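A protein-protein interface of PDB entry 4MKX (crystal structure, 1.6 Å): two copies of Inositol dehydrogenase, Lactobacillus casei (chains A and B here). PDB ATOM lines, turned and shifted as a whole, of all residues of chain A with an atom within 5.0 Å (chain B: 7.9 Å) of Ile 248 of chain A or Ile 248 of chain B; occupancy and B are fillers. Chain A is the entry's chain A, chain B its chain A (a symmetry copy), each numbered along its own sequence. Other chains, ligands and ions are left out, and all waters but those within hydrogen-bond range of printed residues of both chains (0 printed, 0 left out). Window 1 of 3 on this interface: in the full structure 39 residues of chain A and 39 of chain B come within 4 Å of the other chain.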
ATOM      1  N   LEU A 164      -8.953  -8.460   7.749  1.00  0.00           N
ATOM      2  CA  LEU A 164     -10.361  -8.088   7.699  1.00  0.00           C
ATOM      3  C   LEU A 164     -11.231  -9.338   7.691  1.00  0.00           C
ATOM      4  O   LEU A 164     -10.924 -10.313   7.012  1.00  0.00           O
ATOM      5  CB  LEU A 164     -10.650  -7.256   6.438  1.00  0.00           C
ATOM      6  CG  LEU A 164     -12.066  -6.678   6.281  1.00  0.00           C
ATOM      7  CD1 LEU A 164     -11.975  -5.372   5.524  1.00  0.00           C
ATOM      8  CD2 LEU A 164     -12.980  -7.629   5.521  1.00  0.00           C
ATOM      9  N   ILE A 165     -12.318  -9.296   8.450  1.00  0.00           N
ATOM     10  CA  ILE A 165     -13.311 -10.350   8.354  1.00  0.00           C
ATOM     11  C   ILE A 165     -14.658  -9.722   8.021  1.00  0.00           C
ATOM     12  O   ILE A 165     -15.059  -8.744   8.633  1.00  0.00           O
ATOM     13  CB  ILE A 165     -13.413 -11.155   9.657  1.00  0.00           C
ATOM     14  CG1 ILE A 165     -12.122 -11.928   9.876  1.00  0.00           C
ATOM     15  CG2 ILE A 165     -14.560 -12.156   9.556  1.00  0.00           C
ATOM     16  CD1 ILE A 165     -12.152 -12.805  11.121  1.00  0.00           C
ATOM     17  N   ARG A 166     -15.340 -10.280   7.022  1.00  0.00           N
ATOM     18  CA  ARG A 166     -16.682  -9.829   6.667  1.00  0.00           C
ATOM     19  C   ARG A 166     -17.599 -11.016   6.906  1.00  0.00           C
ATOM     20  O   ARG A 166     -17.328 -12.111   6.429  1.00  0.00           O
ATOM     21  CB  ARG A 166     -16.759  -9.421   5.193  1.00  0.00           C
ATOM     22  CG  ARG A 166     -18.185  -9.108   4.745  1.00  0.00           C
ATOM     23  CD  ARG A 166     -18.275  -8.663   3.258  1.00  0.00           C
ATOM     24  NE  ARG A 166     -17.774  -9.666   2.318  1.00  0.00           N
ATOM     25  CZ  ARG A 166     -18.494 -10.670   1.836  1.00  0.00           C
ATOM     26  NH1 ARG A 166     -19.756 -10.822   2.223  1.00  0.00           N
ATOM     27  NH2 ARG A 166     -17.956 -11.541   0.991  1.00  0.00           N
ATOM     28  N   SER A 167     -18.655 -10.819   7.677  1.00  0.00           N
ATOM     29  CA  SER A 167     -19.595 -11.910   7.898  1.00  0.00           C
ATOM     30  C   SER A 167     -21.033 -11.447   7.714  1.00  0.00           C
ATOM     31  O   SER A 167     -21.427 -10.381   8.196  1.00  0.00           O
ATOM     32  CB  SER A 167     -19.365 -12.541   9.284  1.00  0.00           C
ATOM     33  OG  SER A 167     -19.799 -13.893   9.288  1.00  0.00           O
ATOM     34  N   TYR A 168     -21.809 -12.237   6.970  1.00  0.00           N
ATOM     35  CA  TYR A 168     -23.197 -11.922   6.696  1.00  0.00           C
ATOM     36  C   TYR A 168     -24.052 -13.017   7.286  1.00  0.00           C
ATOM     37  O   TYR A 168     -23.761 -14.200   7.092  1.00  0.00           O
ATOM     38  CB  TYR A 168     -23.454 -11.972   5.188  1.00  0.00           C
ATOM     39  CG  TYR A 168     -23.024 -10.780   4.364  1.00  0.00           C
ATOM     40  CD1 TYR A 168     -22.142  -9.817   4.844  1.00  0.00           C
ATOM     41  CD2 TYR A 168     -23.513 -10.633   3.081  1.00  0.00           C
ATOM     42  CE1 TYR A 168     -21.772  -8.727   4.049  1.00  0.00           C
ATOM     43  CE2 TYR A 168     -23.144  -9.566   2.284  1.00  0.00           C
ATOM     44  CZ  TYR A 168     -22.288  -8.619   2.764  1.00  0.00           C
ATOM     45  OH  TYR A 168     -21.955  -7.561   1.952  1.00  0.00           O
ATOM     46  N   ALA A 236     -26.026  -2.988   9.000  1.00  0.00           N
ATOM     47  CA  ALA A 236     -24.638  -3.193   8.691  1.00  0.00           C
ATOM     48  C   ALA A 236     -23.798  -2.554   9.778  1.00  0.00           C
ATOM     49  O   ALA A 236     -24.214  -1.577  10.408  1.00  0.00           O
ATOM     50  CB  ALA A 236     -24.307  -2.590   7.327  1.00  0.00           C
ATOM     51  N   ALA A 237     -22.607  -3.097   9.985  1.00  0.00           N
ATOM     52  CA  ALA A 237     -21.730  -2.580  11.012  1.00  0.00           C
ATOM     53  C   ALA A 237     -20.281  -2.640  10.594  1.00  0.00           C
ATOM     54  O   ALA A 237     -19.853  -3.550   9.869  1.00  0.00           O
ATOM     55  CB  ALA A 237     -21.937  -3.359  12.313  1.00  0.00           C
ATOM     56  N   LEU A 238     -19.510  -1.668  11.074  1.00  0.00           N
ATOM     57  CA  LEU A 238     -18.073  -1.688  10.899  1.00  0.00           C
ATOM     58  C   LEU A 238     -17.467  -1.730  12.296  1.00  0.00           C
ATOM     59  O   LEU A 238     -17.930  -1.036  13.194  1.00  0.00           O
ATOM     60  CB  LEU A 238     -17.614  -0.431  10.167  1.00  0.00           C
ATOM     61  CG  LEU A 238     -16.127  -0.296   9.877  1.00  0.00           C
ATOM     62  CD1 LEU A 238     -15.633  -1.437   8.995  1.00  0.00           C
ATOM     63  CD2 LEU A 238     -15.901   1.069   9.220  1.00  0.00           C
ATOM     64  N   MET A 246      -9.956  -5.202  11.136  1.00  0.00           N
ATOM     65  CA  MET A 246     -11.229  -4.665  10.718  1.00  0.00           C
ATOM     66  C   MET A 246     -12.237  -5.783  10.590  1.00  0.00           C
ATOM     67  O   MET A 246     -11.888  -6.890  10.217  1.00  0.00           O
ATOM     68  CB  MET A 246     -11.056  -3.951   9.385  1.00  0.00           C
ATOM     69  CG  MET A 246     -10.053  -2.826   9.478  1.00  0.00           C
ATOM     70  SD  MET A 246      -9.692  -2.083   7.890  1.00  0.00           S
ATOM     71  CE  MET A 246      -8.636  -3.298   7.157  1.00  0.00           C
ATOM     72  N   ALA A 247     -13.488  -5.476  10.895  1.00  0.00           N
ATOM     73  CA  ALA A 247     -14.557  -6.439  10.654  1.00  0.00           C
ATOM     74  C   ALA A 247     -15.789  -5.730  10.139  1.00  0.00           C
ATOM     75  O   ALA A 247     -16.076  -4.598  10.504  1.00  0.00           O
ATOM     76  CB  ALA A 247     -14.886  -7.238  11.912  1.00  0.00           C
ATOM     77  N   ILE A 248     -16.506  -6.416   9.258  1.00  0.00           N
ATOM     78  CA  ILE A 248     -17.721  -5.889   8.666  1.00  0.00           C
ATOM     79  C   ILE A 248     -18.819  -6.902   8.913  1.00  0.00           C
ATOM     80  O   ILE A 248     -18.618  -8.098   8.684  1.00  0.00           O
ATOM     81  CB  ILE A 248     -17.544  -5.733   7.147  1.00  0.00           C
ATOM     82  CG1 ILE A 248     -16.477  -4.679   6.856  1.00  0.00           C
ATOM     83  CG2 ILE A 248     -18.860  -5.339   6.489  1.00  0.00           C
ATOM     84  CD1 ILE A 248     -16.121  -4.572   5.410  1.00  0.00           C
ATOM     85  N   LEU A 249     -19.967  -6.446   9.405  1.00  0.00           N
ATOM     86  CA  LEU A 249     -21.106  -7.343   9.588  1.00  0.00           C
ATOM     87  C   LEU A 249     -22.289  -6.870   8.772  1.00  0.00           C
ATOM     88  O   LEU A 249     -22.514  -5.678   8.644  1.00  0.00           O
ATOM     89  CB  LEU A 249     -21.540  -7.378  11.053  1.00  0.00           C
ATOM     90  CG  LEU A 249     -20.567  -7.935  12.074  1.00  0.00           C
ATOM     91  CD1 LEU A 249     -21.252  -7.973  13.436  1.00  0.00           C
ATOM     92  CD2 LEU A 249     -20.114  -9.319  11.654  1.00  0.00           C
ATOM     93  N   VAL A 250     -23.053  -7.808   8.228  1.00  0.00           N
ATOM     94  CA  VAL A 250     -24.371  -7.471   7.703  1.00  0.00           C
ATOM     95  C   VAL A 250     -25.337  -8.493   8.277  1.00  0.00           C
ATOM     96  O   VAL A 250     -25.036  -9.684   8.319  1.00  0.00           O
ATOM     97  CB  VAL A 250     -24.432  -7.485   6.165  1.00  0.00           C
ATOM     98  CG1 VAL A 250     -25.881  -7.363   5.705  1.00  0.00           C
ATOM     99  CG2 VAL A 250     -23.623  -6.342   5.584  1.00  0.00           C
ATOM    100  N   LEU B 164     -28.426  -1.927   0.091  1.00  0.00           N
ATOM    101  CA  LEU B 164     -27.017  -1.920   0.462  1.00  0.00           C
ATOM    102  C   LEU B 164     -26.151  -2.140  -0.772  1.00  0.00           C
ATOM    103  O   LEU B 164     -26.465  -2.971  -1.619  1.00  0.00           O
ATOM    104  CB  LEU B 164     -26.729  -3.024   1.492  1.00  0.00           C
ATOM    105  CG  LEU B 164     -25.311  -3.088   2.083  1.00  0.00           C
ATOM    106  CD1 LEU B 164     -25.399  -3.616   3.499  1.00  0.00           C
ATOM    107  CD2 LEU B 164     -24.404  -4.000   1.270  1.00  0.00           C
ATOM    108  N   ILE B 165     -25.062  -1.389  -0.861  1.00  0.00           N
ATOM    109  CA  ILE B 165     -24.073  -1.664  -1.888  1.00  0.00           C
ATOM    110  C   ILE B 165     -22.726  -1.892  -1.217  1.00  0.00           C
ATOM    111  O   ILE B 165     -22.318  -1.127  -0.357  1.00  0.00           O
ATOM    112  CB  ILE B 165     -23.970  -0.514  -2.899  1.00  0.00           C
ATOM    113  CG1 ILE B 165     -25.263  -0.423  -3.694  1.00  0.00           C
ATOM    114  CG2 ILE B 165     -22.828  -0.786  -3.874  1.00  0.00           C
ATOM    115  CD1 ILE B 165     -25.233   0.658  -4.767  1.00  0.00           C
ATOM    116  N   ARG B 166     -22.049  -2.974  -1.602  1.00  0.00           N
ATOM    117  CA  ARG B 166     -20.706  -3.253  -1.104  1.00  0.00           C
ATOM    118  C   ARG B 166     -19.793  -3.220  -2.317  1.00  0.00           C
ATOM    119  O   ARG B 166     -20.070  -3.872  -3.315  1.00  0.00           O
ATOM    120  CB  ARG B 166     -20.633  -4.639  -0.455  1.00  0.00           C
ATOM    121  CG  ARG B 166     -19.207  -5.033  -0.076  1.00  0.00           C
ATOM    122  CD  ARG B 166     -19.120  -6.426   0.612  1.00  0.00           C
ATOM    123  NE  ARG B 166     -19.628  -7.518  -0.218  1.00  0.00           N
ATOM    124  CZ  ARG B 166     -18.913  -8.164  -1.130  1.00  0.00           C
ATOM    125  NH1 ARG B 166     -17.651  -7.813  -1.349  1.00  0.00           N
ATOM    126  NH2 ARG B 166     -19.458  -9.140  -1.845  1.00  0.00           N
ATOM    127  N   SER B 167     -18.734  -2.431  -2.255  1.00  0.00           N
ATOM    128  CA  SER B 167     -17.798  -2.399  -3.370  1.00  0.00           C
ATOM    129  C   SER B 167     -16.358  -2.509  -2.888  1.00  0.00           C
ATOM    130  O   SER B 167     -15.959  -1.857  -1.918  1.00  0.00           O
ATOM    131  CB  SER B 167     -18.025  -1.138  -4.223  1.00  0.00           C
ATOM    132  OG  SER B 167     -17.597  -1.362  -5.559  1.00  0.00           O
ATOM    133  N   TYR B 168     -15.588  -3.378  -3.544  1.00  0.00           N
ATOM    134  CA  TYR B 168     -14.200  -3.601  -3.193  1.00  0.00           C
ATOM    135  C   TYR B 168     -13.347  -3.206  -4.374  1.00  0.00           C
ATOM    136  O   TYR B 168     -13.643  -3.593  -5.507  1.00  0.00           O
ATOM    137  CB  TYR B 168     -13.948  -5.097  -2.991  1.00  0.00           C
ATOM    138  CG  TYR B 168     -14.375  -5.708  -1.677  1.00  0.00           C
ATOM    139  CD1 TYR B 168     -15.252  -5.070  -0.804  1.00  0.00           C
ATOM    140  CD2 TYR B 168     -13.890  -6.950  -1.318  1.00  0.00           C
ATOM    141  CE1 TYR B 168     -15.621  -5.670   0.405  1.00  0.00           C
ATOM    142  CE2 TYR B 168     -14.258  -7.556  -0.132  1.00  0.00           C
ATOM    143  CZ  TYR B 168     -15.109  -6.920   0.725  1.00  0.00           C
ATOM    144  OH  TYR B 168     -15.440  -7.543   1.904  1.00  0.00           O
ATOM    145  N   ASP B 199     -15.562   3.531  -6.942  1.00  0.00           N
ATOM    146  CA  ASP B 199     -16.600   2.907  -6.134  1.00  0.00           C
ATOM    147  C   ASP B 199     -17.644   3.925  -5.682  1.00  0.00           C
ATOM    148  O   ASP B 199     -18.842   3.649  -5.707  1.00  0.00           O
ATOM    149  CB  ASP B 199     -15.978   2.206  -4.927  1.00  0.00           C
ATOM    150  CG  ASP B 199     -15.111   1.032  -5.323  1.00  0.00           C
ATOM    151  OD1 ASP B 199     -15.606   0.138  -6.042  1.00  0.00           O
ATOM    152  OD2 ASP B 199     -13.932   1.002  -4.920  1.00  0.00           O
ATOM    153  N   ILE B 203     -21.667   3.850  -6.659  1.00  0.00           N
ATOM    154  CA  ILE B 203     -22.740   3.967  -5.682  1.00  0.00           C
ATOM    155  C   ILE B 203     -23.743   5.054  -6.098  1.00  0.00           C
ATOM    156  O   ILE B 203     -24.964   4.813  -6.153  1.00  0.00           O
ATOM    157  CB  ILE B 203     -22.155   4.206  -4.291  1.00  0.00           C
ATOM    158  CG1 ILE B 203     -21.517   2.906  -3.796  1.00  0.00           C
ATOM    159  CG2 ILE B 203     -23.232   4.650  -3.306  1.00  0.00           C
ATOM    160  CD1 ILE B 203     -20.474   3.102  -2.724  1.00  0.00           C
ATOM    161  N   ILE B 217     -11.834   3.163   8.569  1.00  0.00           N
ATOM    162  CA  ILE B 217     -10.715   2.676   9.356  1.00  0.00           C
ATOM    163  C   ILE B 217      -9.725   1.983   8.434  1.00  0.00           C
ATOM    164  O   ILE B 217     -10.026   1.696   7.280  1.00  0.00           O
ATOM    165  CB  ILE B 217     -11.159   1.711  10.485  1.00  0.00           C
ATOM    166  CG1 ILE B 217     -11.832   0.456   9.922  1.00  0.00           C
ATOM    167  CG2 ILE B 217     -12.099   2.406  11.463  1.00  0.00           C
ATOM    168  CD1 ILE B 217     -12.339  -0.483  11.037  1.00  0.00           C
ATOM    169  N   GLY B 235      -8.124  -0.504   3.787  1.00  0.00           N
ATOM    170  CA  GLY B 235      -9.044   0.317   4.539  1.00  0.00           C
ATOM    171  C   GLY B 235     -10.454  -0.134   4.277  1.00  0.00           C
ATOM    172  O   GLY B 235     -10.756  -0.747   3.248  1.00  0.00           O
ATOM    173  N   ALA B 236     -11.328   0.155   5.220  1.00  0.00           N
ATOM    174  CA  ALA B 236     -12.717  -0.179   5.074  1.00  0.00           C
ATOM    175  C   ALA B 236     -13.551   1.003   5.525  1.00  0.00           C
ATOM    176  O   ALA B 236     -13.129   1.786   6.382  1.00  0.00           O
ATOM    177  CB  ALA B 236     -13.051  -1.421   5.899  1.00  0.00           C
ATOM    178  N   ALA B 237     -14.744   1.121   4.959  1.00  0.00           N
ATOM    179  CA  ALA B 237     -15.615   2.224   5.300  1.00  0.00           C
ATOM    180  C   ALA B 237     -17.066   1.807   5.315  1.00  0.00           C
ATOM    181  O   ALA B 237     -17.500   0.942   4.541  1.00  0.00           O
ATOM    182  CB  ALA B 237     -15.407   3.375   4.314  1.00  0.00           C
ATOM    183  N   LEU B 238     -17.831   2.446   6.196  1.00  0.00           N
ATOM    184  CA  LEU B 238     -19.269   2.276   6.210  1.00  0.00           C
ATOM    185  C   LEU B 238     -19.871   3.649   5.938  1.00  0.00           C
ATOM    186  O   LEU B 238     -19.402   4.648   6.469  1.00  0.00           O
ATOM    187  CB  LEU B 238     -19.726   1.767   7.573  1.00  0.00           C
ATOM    188  CG  LEU B 238     -21.213   1.509   7.760  1.00  0.00           C
ATOM    189  CD1 LEU B 238     -21.714   0.450   6.784  1.00  0.00           C
ATOM    190  CD2 LEU B 238     -21.436   1.090   9.216  1.00  0.00           C
ATOM    191  N   MET B 239     -20.890   3.688   5.095  1.00  0.00           N
ATOM    192  CA  MET B 239     -21.459   4.956   4.658  1.00  0.00           C
ATOM    193  C   MET B 239     -22.965   4.887   4.740  1.00  0.00           C
ATOM    194  O   MET B 239     -23.583   3.878   4.401  1.00  0.00           O
ATOM    195  CB  MET B 239     -21.024   5.253   3.219  1.00  0.00           C
ATOM    196  CG  MET B 239     -19.532   5.177   3.033  1.00  0.00           C
ATOM    197  SD  MET B 239     -18.998   5.863   1.461  1.00  0.00           S
ATOM    198  CE  MET B 239     -19.864   4.773   0.356  1.00  0.00           C
ATOM    199  N   GLN B 240     -23.568   5.981   5.189  1.00  0.00           N
ATOM    200  CA  GLN B 240     -25.004   6.063   5.230  1.00  0.00           C
ATOM    201  C   GLN B 240     -25.364   7.104   4.190  1.00  0.00           C
ATOM    202  O   GLN B 240     -24.823   8.212   4.207  1.00  0.00           O
ATOM    203  CB  GLN B 240     -25.434   6.556   6.601  1.00  0.00           C
ATOM    204  CG  GLN B 240     -26.920   6.520   6.845  1.00  0.00           C
ATOM    205  CD  GLN B 240     -27.218   6.705   8.329  1.00  0.00           C
ATOM    206  OE1 GLN B 240     -26.728   7.648   8.953  1.00  0.00           O
ATOM    207  NE2 GLN B 240     -27.990   5.796   8.897  1.00  0.00           N
ATOM    208  N   LEU B 241     -26.253   6.737   3.278  1.00  0.00           N
ATOM    209  CA  LEU B 241     -26.639   7.664   2.210  1.00  0.00           C
ATOM    210  C   LEU B 241     -27.844   8.484   2.676  1.00  0.00           C
ATOM    211  O   LEU B 241     -28.384   8.235   3.754  1.00  0.00           O
ATOM    212  CB  LEU B 241     -26.952   6.902   0.929  1.00  0.00           C
ATOM    213  CG  LEU B 241     -25.779   6.482   0.032  1.00  0.00           C
ATOM    214  CD1 LEU B 241     -24.703   5.671   0.753  1.00  0.00           C
ATOM    215  CD2 LEU B 241     -26.307   5.714  -1.172  1.00  0.00           C
ATOM    216  N   THR B 245     -29.784   4.582   2.978  1.00  0.00           N
ATOM    217  CA  THR B 245     -29.194   3.473   2.215  1.00  0.00           C
ATOM    218  C   THR B 245     -27.820   3.211   2.765  1.00  0.00           C
ATOM    219  O   THR B 245     -27.123   4.140   3.182  1.00  0.00           O
ATOM    220  CB  THR B 245     -29.028   3.825   0.716  1.00  0.00           C
ATOM    221  OG1 THR B 245     -30.315   3.987   0.130  1.00  0.00           O
ATOM    222  CG2 THR B 245     -28.277   2.719  -0.039  1.00  0.00           C
ATOM    223  N   MET B 246     -27.399   1.953   2.734  1.00  0.00           N
ATOM    224  CA  MET B 246     -26.125   1.626   3.328  1.00  0.00           C
ATOM    225  C   MET B 246     -25.122   1.309   2.245  1.00  0.00           C
ATOM    226  O   MET B 246     -25.476   0.758   1.217  1.00  0.00           O
ATOM    227  CB  MET B 246     -26.300   0.432   4.256  1.00  0.00           C
ATOM    228  CG  MET B 246     -27.298   0.716   5.353  1.00  0.00           C
ATOM    229  SD  MET B 246     -27.662  -0.724   6.352  1.00  0.00           S
ATOM    230  CE  MET B 246     -28.725  -1.645   5.281  1.00  0.00           C
ATOM    231  N   ALA B 247     -23.869   1.656   2.491  1.00  0.00           N
ATOM    232  CA  ALA B 247     -22.805   1.253   1.579  1.00  0.00           C
ATOM    233  C   ALA B 247     -21.571   0.859   2.360  1.00  0.00           C
ATOM    234  O   ALA B 247     -21.279   1.407   3.415  1.00  0.00           O
ATOM    235  CB  ALA B 247     -22.474   2.358   0.579  1.00  0.00           C
ATOM    236  N   ILE B 248     -20.860  -0.127   1.829  1.00  0.00           N
ATOM    237  CA  ILE B 248     -19.645  -0.628   2.443  1.00  0.00           C
ATOM    238  C   ILE B 248     -18.551  -0.557   1.400  1.00  0.00           C
ATOM    239  O   ILE B 248     -18.757  -0.982   0.259  1.00  0.00           O
ATOM    240  CB  ILE B 248     -19.826  -2.098   2.852  1.00  0.00           C
ATOM    241  CG1 ILE B 248     -20.890  -2.204   3.943  1.00  0.00           C
ATOM    242  CG2 ILE B 248     -18.511  -2.686   3.346  1.00  0.00           C
ATOM    243  CD1 ILE B 248     -21.251  -3.610   4.292  1.00  0.00           C
ATOM    244  N   LEU B 249     -17.399   0.000   1.763  1.00  0.00           N
ATOM    245  CA  LEU B 249     -16.263   0.026   0.844  1.00  0.00           C
ATOM    246  C   LEU B 249     -15.081  -0.705   1.444  1.00  0.00           C
ATOM    247  O   LEU B 249     -14.852  -0.633   2.639  1.00  0.00           O
ATOM    248  CB  LEU B 249     -15.824   1.462   0.564  1.00  0.00           C
ATOM    249  CG  LEU B 249     -16.796   2.379  -0.153  1.00  0.00           C
ATOM    250  CD1 LEU B 249     -16.107   3.713  -0.422  1.00  0.00           C
ATOM    251  CD2 LEU B 249     -17.255   1.736  -1.446  1.00  0.00           C
ATOM    252  N   VAL B 250     -14.322  -1.401   0.608  1.00  0.00           N
ATOM    253  CA  VAL B 250     -13.005  -1.868   1.023  1.00  0.00           C
ATOM    254  C   VAL B 250     -12.041  -1.477  -0.084  1.00  0.00           C
ATOM    255  O   VAL B 250     -12.347  -1.633  -1.264  1.00  0.00           O
ATOM    256  CB  VAL B 250     -12.949  -3.386   1.266  1.00  0.00           C
ATOM    257  CG1 VAL B 250     -11.501  -3.825   1.459  1.00  0.00           C
ATOM    258  CG2 VAL B 250     -13.755  -3.764   2.493  1.00  0.00           C
ATOM    259  N   ALA B 251     -10.902  -0.913   0.298  1.00  0.00           N
ATOM    260  CA  ALA B 251      -9.873  -0.522  -0.658  1.00  0.00           C
ATOM    261  C   ALA B 251      -8.573  -1.110  -0.164  1.00  0.00           C
ATOM    262  O   ALA B 251      -8.332  -1.198   1.037  1.00  0.00           O
ATOM    263  CB  ALA B 251      -9.763   0.984  -0.753  1.00  0.00           C
ATOM    264  N   GLU B 262     -15.004  -5.698  -7.218  1.00  0.00           N
ATOM    265  CA  GLU B 262     -16.236  -6.449  -7.052  1.00  0.00           C
ATOM    266  C   GLU B 262     -17.270  -5.474  -6.518  1.00  0.00           C
ATOM    267  O   GLU B 262     -16.955  -4.639  -5.673  1.00  0.00           O
ATOM    268  CB  GLU B 262     -16.036  -7.581  -6.034  1.00  0.00           C
ATOM    269  CG  GLU B 262     -17.316  -8.380  -5.714  1.00  0.00           C
ATOM    270  CD  GLU B 262     -17.186  -9.248  -4.495  1.00  0.00           C
ATOM    271  OE1 GLU B 262     -16.143  -9.164  -3.800  1.00  0.00           O
ATOM    272  OE2 GLU B 262     -18.136 -10.018  -4.201  1.00  0.00           O
ATOM    273  N   THR B 263     -18.491  -5.551  -7.041  1.00  0.00           N
ATOM    274  CA  THR B 263     -19.577  -4.719  -6.529  1.00  0.00           C
ATOM    275  C   THR B 263     -20.798  -5.578  -6.300  1.00  0.00           C
ATOM    276  O   THR B 263     -21.256  -6.283  -7.197  1.00  0.00           O
ATOM    277  CB  THR B 263     -19.911  -3.593  -7.512  1.00  0.00           C
ATOM    278  OG1 THR B 263     -18.741  -2.790  -7.689  1.00  0.00           O
ATOM    279  CG2 THR B 263     -21.008  -2.701  -6.951  1.00  0.00           C
ATOM    280  N   GLU B 264     -21.333  -5.496  -5.086  1.00  0.00           N
ATOM    281  CA  GLU B 264     -22.498  -6.260  -4.684  1.00  0.00           C
ATOM    282  C   GLU B 264     -23.638  -5.286  -4.436  1.00  0.00           C
ATOM    283  O   GLU B 264     -23.449  -4.258  -3.780  1.00  0.00           O
ATOM    284  CB  GLU B 264     -22.169  -6.982  -3.380  1.00  0.00           C
ATOM    285  CG  GLU B 264     -23.334  -7.539  -2.632  1.00  0.00           C
ATOM    286  CD  GLU B 264     -22.886  -8.078  -1.302  1.00  0.00           C
ATOM    287  OE1 GLU B 264     -22.324  -9.195  -1.288  1.00  0.00           O
ATOM    288  OE2 GLU B 264     -23.042  -7.379  -0.278  1.00  0.00           O
ATOM    289  N   ILE B 266     -27.527  -5.271  -2.930  1.00  0.00           N
ATOM    290  CA  ILE B 266     -28.623  -5.966  -2.268  1.00  0.00           C
ATOM    291  C   ILE B 266     -29.879  -5.115  -2.392  1.00  0.00           C
ATOM    292  O   ILE B 266     -29.866  -3.931  -2.052  1.00  0.00           O
ATOM    293  CB  ILE B 266     -28.326  -6.179  -0.787  1.00  0.00           C
ATOM    294  CG1 ILE B 266     -27.021  -6.970  -0.634  1.00  0.00           C
ATOM    295  CG2 ILE B 266     -29.467  -6.949  -0.145  1.00  0.00           C
ATOM    296  CD1 ILE B 266     -26.662  -7.296   0.803  1.00  0.00           C
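Of the 26 printed residues of chain B, 10 touch a printed residue of chain A. Hydrophobic or aromatic side chains of chain B within 4 Å of the printed part of chain A: Leu 164, Tyr 168, Ile 217, Ala 236, Leu 238, Met 246, Ile 248 and Val 250. Along chain B the printed residues that touch a printed residue of chain A span positions 164 to 264.
Ile 248 of chain B touches just these residues of chain A: Ile 248 (3.7 Å) and Val 250 (3.8 Å). Of the printed residues of chain A, Glu 264 of chain B touches Tyr 168. Printed residues of chain A within 4 Å of Val 250 of chain B: Leu 164 and Ile 248. Of the printed residues of chain A, Tyr 168 of chain B touches Arg 166. Of the printed residues of chain B, Tyr 168 of chain A touches Arg 166 and Glu 264. Met 239 of chain B touches none of the printed residues of chain A. Gly 235 of chain B touches none of the printed residues of chain A. The nearest residue of chain B that does not touch Ile 248 of chain A is Ala 236 of chain B (4.4 Å).
The side-chain hydroxyl (OH) of Tyr 168 of chain A is in hydrogen-bond range of the side-chain carboxylate (OE2) of Glu 264 of chain B (2.5 Å). The guanidinium group of Arg 166 of chain B lies within hydrogen-bond range of the side-chain hydroxyl of Tyr 168 of chain A (3.2 Å). The side-chain hydroxyl of Tyr 168 of chain B lies within hydrogen-bond range of the guanidinium group of Arg 166 of chain A (3.2 Å).
Among the printed residues, merely in contact across the chains: Leu 164 of chain A with Val 250 of chain B, Arg 166 of chain A with Arg 166 of chain B, Ala 236 of chain A with Met 246 of chain B, Leu 238 of chain A with Ile 217 of chain B, Leu 238 of chain A with Leu 238 of chain B, Met 246 of chain A with Ile 217 of chain B, Met 246 of chain A with Ala 236 of chain B, Ile 248 of chain A with Ile 248 of chain B, Ile 248 of chain A with Val 250 of chain B, Val 250 of chain A with Leu 164 of chain B and Val 250 of chain A with Ile 248 of chain B.
Arg 166 of chain A touches Tyr 168 of chain B, and with the chains exchanged Tyr 168 of chain A touches Arg 166 of chain B. Ala 236 of chain A touches Met 246 of chain B, and with the chains exchanged Met 246 of chain A touches Ala 236 of chain B. Leu 238 of chain B touches its own counterpart, Leu 238 of chain A. Ile 248 of chain A touches Val 250 of chain B, and with the chains exchanged Val 250 of chain A touches Ile 248 of chain B. 13 positions are printed for both chains.
The guanidinium group of Arg 166 of chain B lies within salt-bridge range of the side-chain carboxylate of Glu 264 of chain B (2.9 Å). N of Ile 165 of chain B is in hydrogen-bond range of O of Met 246 of chain B. N of Ile 248 of chain A lies within hydrogen-bond range of O of Ile 165 of chain A (2.8 Å). O of Glu 262 of chain B is in hydrogen-bond range of N of Tyr 168 of chain B. The backbone carbonyl oxygen of Leu 164 of chain B sits at hydrogen-bond distance from the backbone NH of Ile 266 of chain B (2.9 Å). The backbone carbonyl oxygen (O) of Met 246 of chain A sits at hydrogen-bond distance from the backbone NH (N) of Ile 165 of chain A, at 3.0 Å.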
